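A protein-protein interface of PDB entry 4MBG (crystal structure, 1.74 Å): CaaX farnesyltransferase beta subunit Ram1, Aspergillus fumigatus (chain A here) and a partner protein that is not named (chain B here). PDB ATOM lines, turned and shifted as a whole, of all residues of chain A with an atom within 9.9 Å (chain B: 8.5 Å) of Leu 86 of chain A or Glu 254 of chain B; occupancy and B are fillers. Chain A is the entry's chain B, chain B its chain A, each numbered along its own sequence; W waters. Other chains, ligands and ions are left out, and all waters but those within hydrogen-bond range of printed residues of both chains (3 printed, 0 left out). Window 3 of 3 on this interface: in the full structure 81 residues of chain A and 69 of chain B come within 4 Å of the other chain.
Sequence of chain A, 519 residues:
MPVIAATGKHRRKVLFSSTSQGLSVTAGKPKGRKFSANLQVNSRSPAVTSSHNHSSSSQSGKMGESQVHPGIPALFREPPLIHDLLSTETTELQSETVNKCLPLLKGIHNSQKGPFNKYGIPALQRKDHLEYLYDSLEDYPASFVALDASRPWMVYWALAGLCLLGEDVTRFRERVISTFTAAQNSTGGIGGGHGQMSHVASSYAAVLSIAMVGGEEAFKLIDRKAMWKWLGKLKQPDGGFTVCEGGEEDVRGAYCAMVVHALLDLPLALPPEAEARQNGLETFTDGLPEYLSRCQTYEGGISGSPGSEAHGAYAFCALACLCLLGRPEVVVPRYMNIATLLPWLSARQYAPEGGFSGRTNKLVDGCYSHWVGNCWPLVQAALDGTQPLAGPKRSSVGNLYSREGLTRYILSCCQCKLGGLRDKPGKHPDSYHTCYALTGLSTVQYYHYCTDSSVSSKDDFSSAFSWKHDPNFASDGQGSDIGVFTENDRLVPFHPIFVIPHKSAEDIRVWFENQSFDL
Among the printed residues, pairs that only touch across the chains: Asp 84 of chain A with Ala 255 of chain B (3.3 Å), Thr 91 of chain A with Arg 195 of chain B (3.3 Å), Ile 82 of chain A with Glu 257 of chain B (3.6 Å), Thr 90 of chain A with Arg 195 of chain B (3.7 Å), Asp 84 of chain A with Asn 258 of chain B (3.7 Å), Leu 86 of chain A with Glu 254 of chain B (3.7 Å), Glu 89 of chain A with Asp 193 of chain B (3.8 Å) and Leu 86 of chain A with Val 194 of chain B (3.8 Å).
Of the 13 printed residues of chain A, 7 touch a printed residue of chain B.
Printed residues of chain A that touch a printed residue of chain B: Ile 82, Asp 84, Leu 86, Thr 88, Glu 89, Thr 90 and Thr 91.
Hydrophobic or aromatic side chains of chain A within 4 Å of the printed part of chain B: Ile 82 and Leu 86.
Of the 22 printed residues of chain B, 8 touch a printed residue of chain A.
Hydrophobic or aromatic side chains of chain B within 4 Å of the printed part of chain A: Val 194, Ala 255 and Pro 256.
Among the printed residues, Asp or Glu carboxylates within 4 Å of a Lys or Arg side-chain nitrogen of the other chain: Asp 84 of chain A with Arg 195 of chain B (3.1 Å).
Water W2 bridges OD2 of Asp 193 of chain B (2.7 Å) and OE1 of Glu 89 of chain A (3.5 Å).
Water W1 lies within hydrogen-bond range of O of Ala 192 of chain B and N of Glu 89 of chain A.
Leu 86 of chain A touches just these residues of chain B: Val 194, Arg 195 and Glu 254.
Glu 254 of chain B touches just one residue of chain A: Leu 86 (3.7 Å).
No residue of chain A comes within 4 Å of Arg 251 of chain B.
Ala 255 of chain B touches one residue of chain A.
Of the printed residues of chain B, Thr 88 of chain A touches Asp 193 and Arg 195.
Of the printed residues of chain A, Asn 258 of chain B touches Asp 84 (3.7 Å).
Printed residues of chain B within 4 Å of Thr 90 of chain A: Asp 193 (2.6 Å) and Arg 195 (3.7 Å).
The nearest residue of chain A that does not touch Glu 254 of chain B is Asp 84 of chain A (5.5 Å).
N of Arg 195 of chain B lies close to OD1 of Asp 193 of chain B.
The side-chain amide nitrogen (ND2) of Asn 258 of chain B sits at hydrogen-bond distance from the backbone carbonyl oxygen (O) of Val 194 of chain B, at 2.9 Å.
NH2 of Arg 195 of chain B lies within salt-bridge range of OD2 of Asp 84 of chain A (3.1 Å).
The guanidinium group (NH1) of Arg 195 of chain B lies within hydrogen-bond range of the side-chain hydroxyl (OG1) of Thr 88 of chain A (3.0 Å).
N of Pro 256 of chain B sits close to OD1 of Asp 84 of chain A.
The backbone NH of Glu 257 of chain B lies within hydrogen-bond range of the side-chain carboxylate of Asp 84 of chain A, 3.0 Å away.
OD2 of Asp 193 of chain B is in hydrogen-bond range of OG1 of Thr 90 of chain A (2.6 Å).
The side-chain carboxylate of Asp 193 of chain B is in hydrogen-bond range of the side-chain hydroxyl of Thr 88 of chain A (2.7 Å).
The backbone carbonyl oxygen of Leu 86 of chain A is in hydrogen-bond range of the guanidinium group of Arg 195 of chain B, 2.9 Å away.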
ATOM      1  N   ILE A  82     -30.504  -4.399  33.499  1.00  0.00           N
ATOM      2  CA  ILE A  82     -29.126  -4.624  33.069  1.00  0.00           C
ATOM      3  C   ILE A  82     -28.993  -4.340  31.589  1.00  0.00           C
ATOM      4  O   ILE A  82     -29.710  -4.908  30.773  1.00  0.00           O
ATOM      5  CB  ILE A  82     -28.656  -6.061  33.344  1.00  0.00           C
ATOM      6  CG1 ILE A  82     -28.670  -6.357  34.847  1.00  0.00           C
ATOM      7  CG2 ILE A  82     -27.242  -6.278  32.771  1.00  0.00           C
ATOM      8  CD1 ILE A  82     -28.275  -7.785  35.160  1.00  0.00           C
ATOM      9  N   HIS A  83     -28.099  -3.436  31.216  1.00  0.00           N
ATOM     10  CA  HIS A  83     -27.901  -3.146  29.795  1.00  0.00           C
ATOM     11  C   HIS A  83     -26.418  -3.028  29.437  1.00  0.00           C
ATOM     12  O   HIS A  83     -25.721  -2.114  29.889  1.00  0.00           O
ATOM     13  CB  HIS A  83     -28.673  -1.884  29.369  1.00  0.00           C
ATOM     14  CG  HIS A  83     -30.057  -2.157  28.855  1.00  0.00           C
ATOM     15  ND1 HIS A  83     -31.160  -2.224  29.680  1.00  0.00           N
ATOM     16  CD2 HIS A  83     -30.517  -2.378  27.599  1.00  0.00           C
ATOM     17  CE1 HIS A  83     -32.238  -2.469  28.958  1.00  0.00           C
ATOM     18  NE2 HIS A  83     -31.877  -2.565  27.691  1.00  0.00           N
ATOM     19  N   ASP A  84     -25.956  -3.971  28.621  1.00  0.00           N
ATOM     20  CA  ASP A  84     -24.570  -4.038  28.139  1.00  0.00           C
ATOM     21  C   ASP A  84     -24.278  -2.789  27.305  1.00  0.00           C
ATOM     22  O   ASP A  84     -25.148  -2.318  26.585  1.00  0.00           O
ATOM     23  CB  ASP A  84     -24.374  -5.226  27.172  1.00  0.00           C
ATOM     24  CG  ASP A  84     -24.377  -6.620  27.845  1.00  0.00           C
ATOM     25  OD1 ASP A  84     -24.123  -6.759  29.050  1.00  0.00           O
ATOM     26  OD2 ASP A  84     -24.600  -7.613  27.104  1.00  0.00           O
ATOM     27  N   LEU A  85     -23.042  -2.294  27.338  1.00  0.00           N
ATOM     28  CA  LEU A  85     -22.652  -1.151  26.501  1.00  0.00           C
ATOM     29  C   LEU A  85     -22.543  -1.490  25.010  1.00  0.00           C
ATOM     30  O   LEU A  85     -22.811  -0.649  24.150  1.00  0.00           O
ATOM     31  CB  LEU A  85     -21.315  -0.570  26.974  1.00  0.00           C
ATOM     32  CG  LEU A  85     -21.269  -0.006  28.391  1.00  0.00           C
ATOM     33  CD1 LEU A  85     -19.912   0.672  28.649  1.00  0.00           C
ATOM     34  CD2 LEU A  85     -22.432   0.961  28.626  1.00  0.00           C
ATOM     35  N   LEU A  86     -22.151  -2.725  24.711  1.00  0.00           N
ATOM     36  CA  LEU A  86     -21.886  -3.132  23.334  1.00  0.00           C
ATOM     37  C   LEU A  86     -23.168  -3.271  22.520  1.00  0.00           C
ATOM     38  O   LEU A  86     -24.060  -4.042  22.886  1.00  0.00           O
ATOM     39  CB  LEU A  86     -21.126  -4.461  23.307  1.00  0.00           C
ATOM     40  CG  LEU A  86     -20.925  -5.030  21.893  1.00  0.00           C
ATOM     41  CD1 LEU A  86     -19.919  -4.191  21.104  1.00  0.00           C
ATOM     42  CD2 LEU A  86     -20.523  -6.509  21.948  1.00  0.00           C
ATOM     43  N   SER A  87     -23.254  -2.525  21.419  1.00  0.00           N
ATOM     44  CA  SER A  87     -24.365  -2.654  20.464  1.00  0.00           C
ATOM     45  C   SER A  87     -24.039  -3.624  19.324  1.00  0.00           C
ATOM     46  O   SER A  87     -22.994  -3.494  18.662  1.00  0.00           O
ATOM     47  CB  SER A  87     -24.695  -1.278  19.872  1.00  0.00           C
ATOM     48  OG  SER A  87     -25.758  -1.342  18.938  1.00  0.00           O
ATOM     49  N   THR A  88     -24.933  -4.588  19.087  1.00  0.00           N
ATOM     50  CA  THR A  88     -24.860  -5.439  17.892  1.00  0.00           C
ATOM     51  C   THR A  88     -26.242  -5.533  17.247  1.00  0.00           C
ATOM     52  O   THR A  88     -27.231  -5.002  17.778  1.00  0.00           O
ATOM     53  CB  THR A  88     -24.373  -6.872  18.212  1.00  0.00           C
ATOM     54  OG1 THR A  88     -25.309  -7.514  19.090  1.00  0.00           O
ATOM     55  CG2 THR A  88     -22.973  -6.859  18.853  1.00  0.00           C
ATOM     56  N   GLU A  89     -26.332  -6.226  16.120  1.00  0.00           N
ATOM     57  CA  GLU A  89     -27.612  -6.340  15.443  1.00  0.00           C
ATOM     58  C   GLU A  89     -28.659  -6.930  16.373  1.00  0.00           C
ATOM     59  O   GLU A  89     -29.799  -6.484  16.371  1.00  0.00           O
ATOM     60  CB  GLU A  89     -27.511  -7.199  14.188  1.00  0.00           C
ATOM     61  CG  GLU A  89     -28.866  -7.481  13.568  1.00  0.00           C
ATOM     62  CD  GLU A  89     -28.765  -8.131  12.216  1.00  0.00           C
ATOM     63  OE1 GLU A  89     -28.407  -9.330  12.156  1.00  0.00           O
ATOM     64  OE2 GLU A  89     -29.039  -7.433  11.214  1.00  0.00           O
ATOM     65  N   THR A  90     -28.269  -7.930  17.160  1.00  0.00           N
ATOM     66  CA  THR A  90     -29.199  -8.539  18.104  1.00  0.00           C
ATOM     67  C   THR A  90     -29.811  -7.477  19.033  1.00  0.00           C
ATOM     68  O   THR A  90     -31.022  -7.457  19.257  1.00  0.00           O
ATOM     69  CB  THR A  90     -28.479  -9.616  18.951  1.00  0.00           C
ATOM     70  OG1 THR A  90     -28.087 -10.685  18.094  1.00  0.00           O
ATOM     71  CG2 THR A  90     -29.407 -10.190  20.048  1.00  0.00           C
ATOM     72  N   THR A  91     -28.975  -6.617  19.617  1.00  0.00           N
ATOM     73  CA  THR A  91     -29.528  -5.658  20.589  1.00  0.00           C
ATOM     74  C   THR A  91     -30.302  -4.548  19.890  1.00  0.00           C
ATOM     75  O   THR A  91     -31.251  -4.002  20.459  1.00  0.00           O
ATOM     76  CB  THR A  91     -28.457  -5.049  21.517  1.00  0.00           C
ATOM     77  OG1 THR A  91     -27.462  -4.395  20.732  1.00  0.00           O
ATOM     78  CG2 THR A  91     -27.822  -6.117  22.352  1.00  0.00           C
ATOM     79  N   GLU A  92     -29.919  -4.236  18.654  1.00  0.00           N
ATOM     80  CA  GLU A  92     -30.668  -3.240  17.873  1.00  0.00           C
ATOM     81  C   GLU A  92     -32.104  -3.720  17.662  1.00  0.00           C
ATOM     82  O   GLU A  92     -33.069  -2.973  17.860  1.00  0.00           O
ATOM     83  CB  GLU A  92     -29.998  -2.984  16.515  1.00  0.00           C
ATOM     84  CG  GLU A  92     -28.664  -2.260  16.613  1.00  0.00           C
ATOM     85  CD  GLU A  92     -27.965  -2.161  15.246  1.00  0.00           C
ATOM     86  OE1 GLU A  92     -28.579  -2.551  14.231  1.00  0.00           O
ATOM     87  OE2 GLU A  92     -26.808  -1.711  15.196  1.00  0.00           O
ATOM     88  N   GLN A  94     -33.658  -6.088  19.365  1.00  0.00           N
ATOM     89  CA  GLN A  94     -34.317  -6.313  20.653  1.00  0.00           C
ATOM     90  C   GLN A  94     -34.840  -4.970  21.175  1.00  0.00           C
ATOM     91  O   GLN A  94     -35.974  -4.875  21.622  1.00  0.00           O
ATOM     92  CB  GLN A  94     -33.348  -6.982  21.651  1.00  0.00           C
ATOM     93  CG  GLN A  94     -33.908  -7.173  23.073  1.00  0.00           C
ATOM     94  CD  GLN A  94     -35.191  -7.989  23.117  1.00  0.00           C
ATOM     95  OE1 GLN A  94     -35.404  -8.905  22.305  1.00  0.00           O
ATOM     96  NE2 GLN A  94     -36.063  -7.653  24.069  1.00  0.00           N
ATOM     97  N   SER A  95     -34.001  -3.937  21.089  1.00  0.00           N
ATOM     98  CA  SER A  95     -34.376  -2.597  21.539  1.00  0.00           C
ATOM     99  C   SER A  95     -35.580  -2.072  20.774  1.00  0.00           C
ATOM    100  O   SER A  95     -36.518  -1.540  21.371  1.00  0.00           O
ATOM    101  CB  SER A  95     -33.198  -1.626  21.377  1.00  0.00           C
ATOM    102  OG  SER A  95     -33.565  -0.321  21.787  1.00  0.00           O
ATOM    103  N   LEU B 190     -19.213 -14.358  15.279  1.00  0.00           N
ATOM    104  CA  LEU B 190     -19.279 -13.919  16.687  1.00  0.00           C
ATOM    105  C   LEU B 190     -18.539 -12.599  16.900  1.00  0.00           C
ATOM    106  O   LEU B 190     -18.842 -11.861  17.826  1.00  0.00           O
ATOM    107  CB  LEU B 190     -18.744 -15.000  17.637  1.00  0.00           C
ATOM    108  CG  LEU B 190     -19.636 -16.256  17.677  1.00  0.00           C
ATOM    109  CD1 LEU B 190     -19.008 -17.249  18.628  1.00  0.00           C
ATOM    110  CD2 LEU B 190     -21.059 -15.903  18.138  1.00  0.00           C
ATOM    111  N   LYS B 191     -17.560 -12.290  16.055  1.00  0.00           N
ATOM    112  CA  LYS B 191     -16.965 -10.947  16.116  1.00  0.00           C
ATOM    113  C   LYS B 191     -17.998  -9.903  15.685  1.00  0.00           C
ATOM    114  O   LYS B 191     -18.115  -8.824  16.306  1.00  0.00           O
ATOM    115  CB  LYS B 191     -15.734 -10.854  15.197  1.00  0.00           C
ATOM    116  CG  LYS B 191     -15.070  -9.473  15.185  1.00  0.00           C
ATOM    117  CD  LYS B 191     -13.727  -9.506  14.415  1.00  0.00           C
ATOM    118  CE  LYS B 191     -13.044  -8.117  14.360  1.00  0.00           C
ATOM    119  NZ  LYS B 191     -13.550  -7.296  13.219  1.00  0.00           N
ATOM    120  N   ALA B 192     -18.733 -10.206  14.617  1.00  0.00           N
ATOM    121  CA  ALA B 192     -19.772  -9.294  14.123  1.00  0.00           C
ATOM    122  C   ALA B 192     -20.915  -9.144  15.121  1.00  0.00           C
ATOM    123  O   ALA B 192     -21.430  -8.024  15.338  1.00  0.00           O
ATOM    124  CB  ALA B 192     -20.305  -9.756  12.750  1.00  0.00           C
ATOM    125  N   ASP B 193     -21.311 -10.250  15.745  1.00  0.00           N
ATOM    126  CA  ASP B 193     -22.394 -10.199  16.752  1.00  0.00           C
ATOM    127  C   ASP B 193     -22.195 -11.330  17.742  1.00  0.00           C
ATOM    128  O   ASP B 193     -22.546 -12.480  17.467  1.00  0.00           O
ATOM    129  CB  ASP B 193     -23.757 -10.339  16.084  1.00  0.00           C
ATOM    130  CG  ASP B 193     -24.928 -10.086  17.039  1.00  0.00           C
ATOM    131  OD1 ASP B 193     -24.713 -10.023  18.266  1.00  0.00           O
ATOM    132  OD2 ASP B 193     -26.072  -9.963  16.553  1.00  0.00           O
ATOM    133  N   VAL B 194     -21.643 -10.993  18.898  1.00  0.00           N
ATOM    134  CA  VAL B 194     -21.290 -11.985  19.908  1.00  0.00           C
ATOM    135  C   VAL B 194     -22.554 -12.677  20.466  1.00  0.00           C
ATOM    136  O   VAL B 194     -22.459 -13.720  21.110  1.00  0.00           O
ATOM    137  CB  VAL B 194     -20.398 -11.349  21.010  1.00  0.00           C
ATOM    138  CG1 VAL B 194     -21.183 -10.285  21.809  1.00  0.00           C
ATOM    139  CG2 VAL B 194     -19.769 -12.426  21.911  1.00  0.00           C
ATOM    140  N   ARG B 195     -23.726 -12.109  20.177  1.00  0.00           N
ATOM    141  CA  ARG B 195     -24.998 -12.659  20.677  1.00  0.00           C
ATOM    142  C   ARG B 195     -25.635 -13.585  19.655  1.00  0.00           C
ATOM    143  O   ARG B 195     -26.811 -13.968  19.793  1.00  0.00           O
ATOM    144  CB  ARG B 195     -25.961 -11.523  20.996  1.00  0.00           C
ATOM    145  CG  ARG B 195     -25.459 -10.716  22.187  1.00  0.00           C
ATOM    146  CD  ARG B 195     -25.793  -9.284  22.033  1.00  0.00           C
ATOM    147  NE  ARG B 195     -25.439  -8.485  23.213  1.00  0.00           N
ATOM    148  CZ  ARG B 195     -24.861  -7.295  23.115  1.00  0.00           C
ATOM    149  NH1 ARG B 195     -24.562  -6.808  21.913  1.00  0.00           N
ATOM    150  NH2 ARG B 195     -24.595  -6.592  24.202  1.00  0.00           N
ATOM    151  N   TRP B 200     -22.893 -19.906  18.195  1.00  0.00           N
ATOM    152  CA  TRP B 200     -22.482 -20.630  19.391  1.00  0.00           C
ATOM    153  C   TRP B 200     -22.889 -22.097  19.321  1.00  0.00           C
ATOM    154  O   TRP B 200     -22.132 -22.981  19.732  1.00  0.00           O
ATOM    155  CB  TRP B 200     -23.103 -19.999  20.645  1.00  0.00           C
ATOM    156  CG  TRP B 200     -22.397 -18.730  21.068  1.00  0.00           C
ATOM    157  CD1 TRP B 200     -22.805 -17.448  20.844  1.00  0.00           C
ATOM    158  CD2 TRP B 200     -21.142 -18.648  21.760  1.00  0.00           C
ATOM    159  NE1 TRP B 200     -21.879 -16.559  21.384  1.00  0.00           N
ATOM    160  CE2 TRP B 200     -20.857 -17.271  21.951  1.00  0.00           C
ATOM    161  CE3 TRP B 200     -20.242 -19.599  22.249  1.00  0.00           C
ATOM    162  CZ2 TRP B 200     -19.699 -16.820  22.593  1.00  0.00           C
ATOM    163  CZ3 TRP B 200     -19.094 -19.145  22.926  1.00  0.00           C
ATOM    164  CH2 TRP B 200     -18.834 -17.771  23.085  1.00  0.00           C
ATOM    165  N   TYR B 247     -12.046 -18.978  26.090  1.00  0.00           N
ATOM    166  CA  TYR B 247     -12.702 -18.264  24.998  1.00  0.00           C
ATOM    167  C   TYR B 247     -14.060 -17.723  25.463  1.00  0.00           C
ATOM    168  O   TYR B 247     -14.404 -16.559  25.231  1.00  0.00           O
ATOM    169  CB  TYR B 247     -12.887 -19.188  23.784  1.00  0.00           C
ATOM    170  CG  TYR B 247     -13.604 -18.537  22.616  1.00  0.00           C
ATOM    171  CD1 TYR B 247     -12.909 -17.768  21.685  1.00  0.00           C
ATOM    172  CD2 TYR B 247     -14.969 -18.696  22.442  1.00  0.00           C
ATOM    173  CE1 TYR B 247     -13.560 -17.168  20.619  1.00  0.00           C
ATOM    174  CE2 TYR B 247     -15.633 -18.100  21.388  1.00  0.00           C
ATOM    175  CZ  TYR B 247     -14.928 -17.343  20.476  1.00  0.00           C
ATOM    176  OH  TYR B 247     -15.592 -16.760  19.433  1.00  0.00           O
ATOM    177  N   SER B 248     -14.822 -18.573  26.125  1.00  0.00           N
ATOM    178  CA  SER B 248     -16.142 -18.176  26.617  1.00  0.00           C
ATOM    179  C   SER B 248     -16.051 -16.999  27.593  1.00  0.00           C
ATOM    180  O   SER B 248     -16.833 -16.041  27.497  1.00  0.00           O
ATOM    181  CB  SER B 248     -16.867 -19.369  27.256  1.00  0.00           C
ATOM    182  OG  SER B 248     -16.966 -20.443  26.310  1.00  0.00           O
ATOM    183  N   GLN B 249     -15.097 -17.058  28.521  1.00  0.00           N
ATOM    184  CA  GLN B 249     -14.922 -15.943  29.461  1.00  0.00           C
ATOM    185  C   GLN B 249     -14.591 -14.651  28.719  1.00  0.00           C
ATOM    186  O   GLN B 249     -15.129 -13.595  29.048  1.00  0.00           O
ATOM    187  CB  GLN B 249     -13.849 -16.229  30.533  1.00  0.00           C
ATOM    188  CG  GLN B 249     -14.220 -17.369  31.464  1.00  0.00           C
ATOM    189  CD  GLN B 249     -13.325 -17.473  32.679  1.00  0.00           C
ATOM    190  OE1 GLN B 249     -12.244 -16.897  32.715  1.00  0.00           O
ATOM    191  NE2 GLN B 249     -13.778 -18.213  33.685  1.00  0.00           N
ATOM    192  N   SER B 250     -13.712 -14.738  27.721  1.00  0.00           N
ATOM    193  CA  SER B 250     -13.313 -13.564  26.953  1.00  0.00           C
ATOM    194  C   SER B 250     -14.493 -12.926  26.254  1.00  0.00           C
ATOM    195  O   SER B 250     -14.613 -11.703  26.229  1.00  0.00           O
ATOM    196  CB  SER B 250     -12.233 -13.902  25.915  1.00  0.00           C
ATOM    197  OG  SER B 250     -11.006 -14.119  26.553  1.00  0.00           O
ATOM    198  N   ARG B 251     -15.369 -13.751  25.681  1.00  0.00           N
ATOM    199  CA  ARG B 251     -16.547 -13.212  25.013  1.00  0.00           C
ATOM    200  C   ARG B 251     -17.542 -12.628  26.031  1.00  0.00           C
ATOM    201  O   ARG B 251     -18.163 -11.586  25.781  1.00  0.00           O
ATOM    202  CB  ARG B 251     -17.223 -14.298  24.167  1.00  0.00           C
ATOM    203  CG  ARG B 251     -16.330 -14.919  23.082  1.00  0.00           C
ATOM    204  CD  ARG B 251     -16.007 -13.944  21.926  1.00  0.00           C
ATOM    205  NE  ARG B 251     -15.031 -12.904  22.234  1.00  0.00           N
ATOM    206  CZ  ARG B 251     -13.720 -13.111  22.363  1.00  0.00           C
ATOM    207  NH1 ARG B 251     -13.226 -14.328  22.243  1.00  0.00           N
ATOM    208  NH2 ARG B 251     -12.899 -12.102  22.630  1.00  0.00           N
ATOM    209  N   ILE B 252     -17.707 -13.310  27.168  1.00  0.00           N
ATOM    210  CA  ILE B 252     -18.603 -12.803  28.213  1.00  0.00           C
ATOM    211  C   ILE B 252     -18.197 -11.376  28.641  1.00  0.00           C
ATOM    212  O   ILE B 252     -19.038 -10.481  28.783  1.00  0.00           O
ATOM    213  CB  ILE B 252     -18.666 -13.761  29.421  1.00  0.00           C
ATOM    214  CG1 ILE B 252     -19.491 -15.014  29.047  1.00  0.00           C
ATOM    215  CG2 ILE B 252     -19.253 -13.037  30.674  1.00  0.00           C
ATOM    216  CD1 ILE B 252     -19.217 -16.242  29.932  1.00  0.00           C
ATOM    217  N   LEU B 253     -16.904 -11.148  28.804  1.00  0.00           N
ATOM    218  CA  LEU B 253     -16.426  -9.833  29.257  1.00  0.00           C
ATOM    219  C   LEU B 253     -16.774  -8.707  28.271  1.00  0.00           C
ATOM    220  O   LEU B 253     -16.894  -7.560  28.669  1.00  0.00           O
ATOM    221  CB  LEU B 253     -14.912  -9.863  29.510  1.00  0.00           C
ATOM    222  CG  LEU B 253     -14.466 -10.702  30.705  1.00  0.00           C
ATOM    223  CD1 LEU B 253     -12.947 -10.912  30.657  1.00  0.00           C
ATOM    224  CD2 LEU B 253     -14.879 -10.039  32.030  1.00  0.00           C
ATOM    225  N   GLU B 254     -16.956  -9.043  26.997  1.00  0.00           N
ATOM    226  CA  GLU B 254     -17.385  -8.060  25.997  1.00  0.00           C
ATOM    227  C   GLU B 254     -18.843  -7.630  26.168  1.00  0.00           C
ATOM    228  O   GLU B 254     -19.215  -6.518  25.769  1.00  0.00           O
ATOM    229  CB  GLU B 254     -17.173  -8.610  24.575  1.00  0.00           C
ATOM    230  CG  GLU B 254     -15.711  -8.903  24.251  1.00  0.00           C
ATOM    231  CD  GLU B 254     -15.519  -9.666  22.955  1.00  0.00           C
ATOM    232  OE1 GLU B 254     -16.512 -10.164  22.391  1.00  0.00           O
ATOM    233  OE2 GLU B 254     -14.364  -9.769  22.505  1.00  0.00           O
ATOM    234  N   ALA B 255     -19.667  -8.517  26.734  1.00  0.00           N
ATOM    235  CA  ALA B 255     -21.114  -8.278  26.902  1.00  0.00           C
ATOM    236  C   ALA B 255     -21.679  -9.274  27.915  1.00  0.00           C
ATOM    237  O   ALA B 255     -22.206 -10.311  27.551  1.00  0.00           O
ATOM    238  CB  ALA B 255     -21.845  -8.405  25.539  1.00  0.00           C
ATOM    239  N   PRO B 256     -21.543  -8.972  29.208  1.00  0.00           N
ATOM    240  CA  PRO B 256     -21.833  -9.963  30.256  1.00  0.00           C
ATOM    241  C   PRO B 256     -23.291 -10.415  30.346  1.00  0.00           C
ATOM    242  O   PRO B 256     -23.514 -11.490  30.902  1.00  0.00           O
ATOM    243  CB  PRO B 256     -21.440  -9.219  31.554  1.00  0.00           C
ATOM    244  CG  PRO B 256     -20.438  -8.204  31.094  1.00  0.00           C
ATOM    245  CD  PRO B 256     -20.950  -7.737  29.757  1.00  0.00           C
ATOM    246  N   GLU B 257     -24.246  -9.635  29.828  1.00  0.00           N
ATOM    247  CA  GLU B 257     -25.663 -10.017  29.921  1.00  0.00           C
ATOM    248  C   GLU B 257     -26.063 -10.926  28.734  1.00  0.00           C
ATOM    249  O   GLU B 257     -27.191 -11.409  28.648  1.00  0.00           O
ATOM    250  CB  GLU B 257     -26.565  -8.777  29.992  1.00  0.00           C
ATOM    251  CG  GLU B 257     -28.058  -9.045  30.301  1.00  0.00           C
ATOM    252  CD  GLU B 257     -28.288  -9.792  31.620  1.00  0.00           C
ATOM    253  OE1 GLU B 257     -27.341  -9.931  32.425  1.00  0.00           O
ATOM    254  OE2 GLU B 257     -29.430 -10.247  31.857  1.00  0.00           O
ATOM    255  N   ASN B 258     -25.110 -11.196  27.856  1.00  0.00           N
ATOM    256  CA  ASN B 258     -25.345 -12.099  26.708  1.00  0.00           C
ATOM    257  C   ASN B 258     -25.452 -13.567  27.175  1.00  0.00           C
ATOM    258  O   ASN B 258     -24.470 -14.161  27.611  1.00  0.00           O
ATOM    259  CB  ASN B 258     -24.162 -11.916  25.756  1.00  0.00           C
ATOM    260  CG  ASN B 258     -24.185 -12.857  24.563  1.00  0.00           C
ATOM    261  OD1 ASN B 258     -25.192 -13.504  24.253  1.00  0.00           O
ATOM    262  ND2 ASN B 258     -23.058 -12.922  23.875  1.00  0.00           N
ATOM    263  N   PRO B 261     -22.883 -17.245  25.586  1.00  0.00           N
ATOM    264  CA  PRO B 261     -21.615 -17.850  26.034  1.00  0.00           C
ATOM    265  C   PRO B 261     -21.742 -18.494  27.413  1.00  0.00           C
ATOM    266  O   PRO B 261     -20.996 -19.424  27.684  1.00  0.00           O
ATOM    267  CB  PRO B 261     -20.638 -16.663  26.072  1.00  0.00           C
ATOM    268  CG  PRO B 261     -21.530 -15.401  26.174  1.00  0.00           C
ATOM    269  CD  PRO B 261     -22.752 -15.795  25.332  1.00  0.00           C
ATOM    270  N   PHE B 282     -15.115 -16.274  38.822  1.00  0.00           N
ATOM    271  CA  PHE B 282     -15.486 -15.525  37.628  1.00  0.00           C
ATOM    272  C   PHE B 282     -16.917 -14.976  37.755  1.00  0.00           C
ATOM    273  O   PHE B 282     -17.162 -13.792  37.514  1.00  0.00           O
ATOM    274  CB  PHE B 282     -15.366 -16.407  36.378  1.00  0.00           C
ATOM    275  CG  PHE B 282     -15.707 -15.700  35.101  1.00  0.00           C
ATOM    276  CD1 PHE B 282     -14.857 -14.729  34.579  1.00  0.00           C
ATOM    277  CD2 PHE B 282     -16.864 -16.028  34.400  1.00  0.00           C
ATOM    278  CE1 PHE B 282     -15.169 -14.074  33.387  1.00  0.00           C
ATOM    279  CE2 PHE B 282     -17.193 -15.373  33.207  1.00  0.00           C
ATOM    280  CZ  PHE B 282     -16.335 -14.402  32.697  1.00  0.00           C
ATOM    281  N   PHE B 286     -18.933 -10.424  38.656  1.00  0.00           N
ATOM    282  CA  PHE B 286     -20.007  -9.628  38.064  1.00  0.00           C
ATOM    283  C   PHE B 286     -21.022  -9.174  39.107  1.00  0.00           C
ATOM    284  O   PHE B 286     -22.004  -8.503  38.777  1.00  0.00           O
ATOM    285  CB  PHE B 286     -20.687 -10.414  36.936  1.00  0.00           C
ATOM    286  CG  PHE B 286     -19.759 -10.751  35.818  1.00  0.00           C
ATOM    287  CD1 PHE B 286     -19.448  -9.808  34.855  1.00  0.00           C
ATOM    288  CD2 PHE B 286     -19.163 -12.000  35.748  1.00  0.00           C
ATOM    289  CE1 PHE B 286     -18.547 -10.104  33.818  1.00  0.00           C
ATOM    290  CE2 PHE B 286     -18.274 -12.310  34.726  1.00  0.00           C
ATOM    291  CZ  PHE B 286     -17.968 -11.357  33.752  1.00  0.00           C
HETATM  292  O   HOH W   1     -23.833  -6.807  14.726  1.00  0.00           O
HETATM  293  O   HOH W   2     -26.459 -11.359  14.231  1.00  0.00           O
HETATM  294  O   HOH W   3     -21.162  -4.664  26.590  1.00  0.00           O
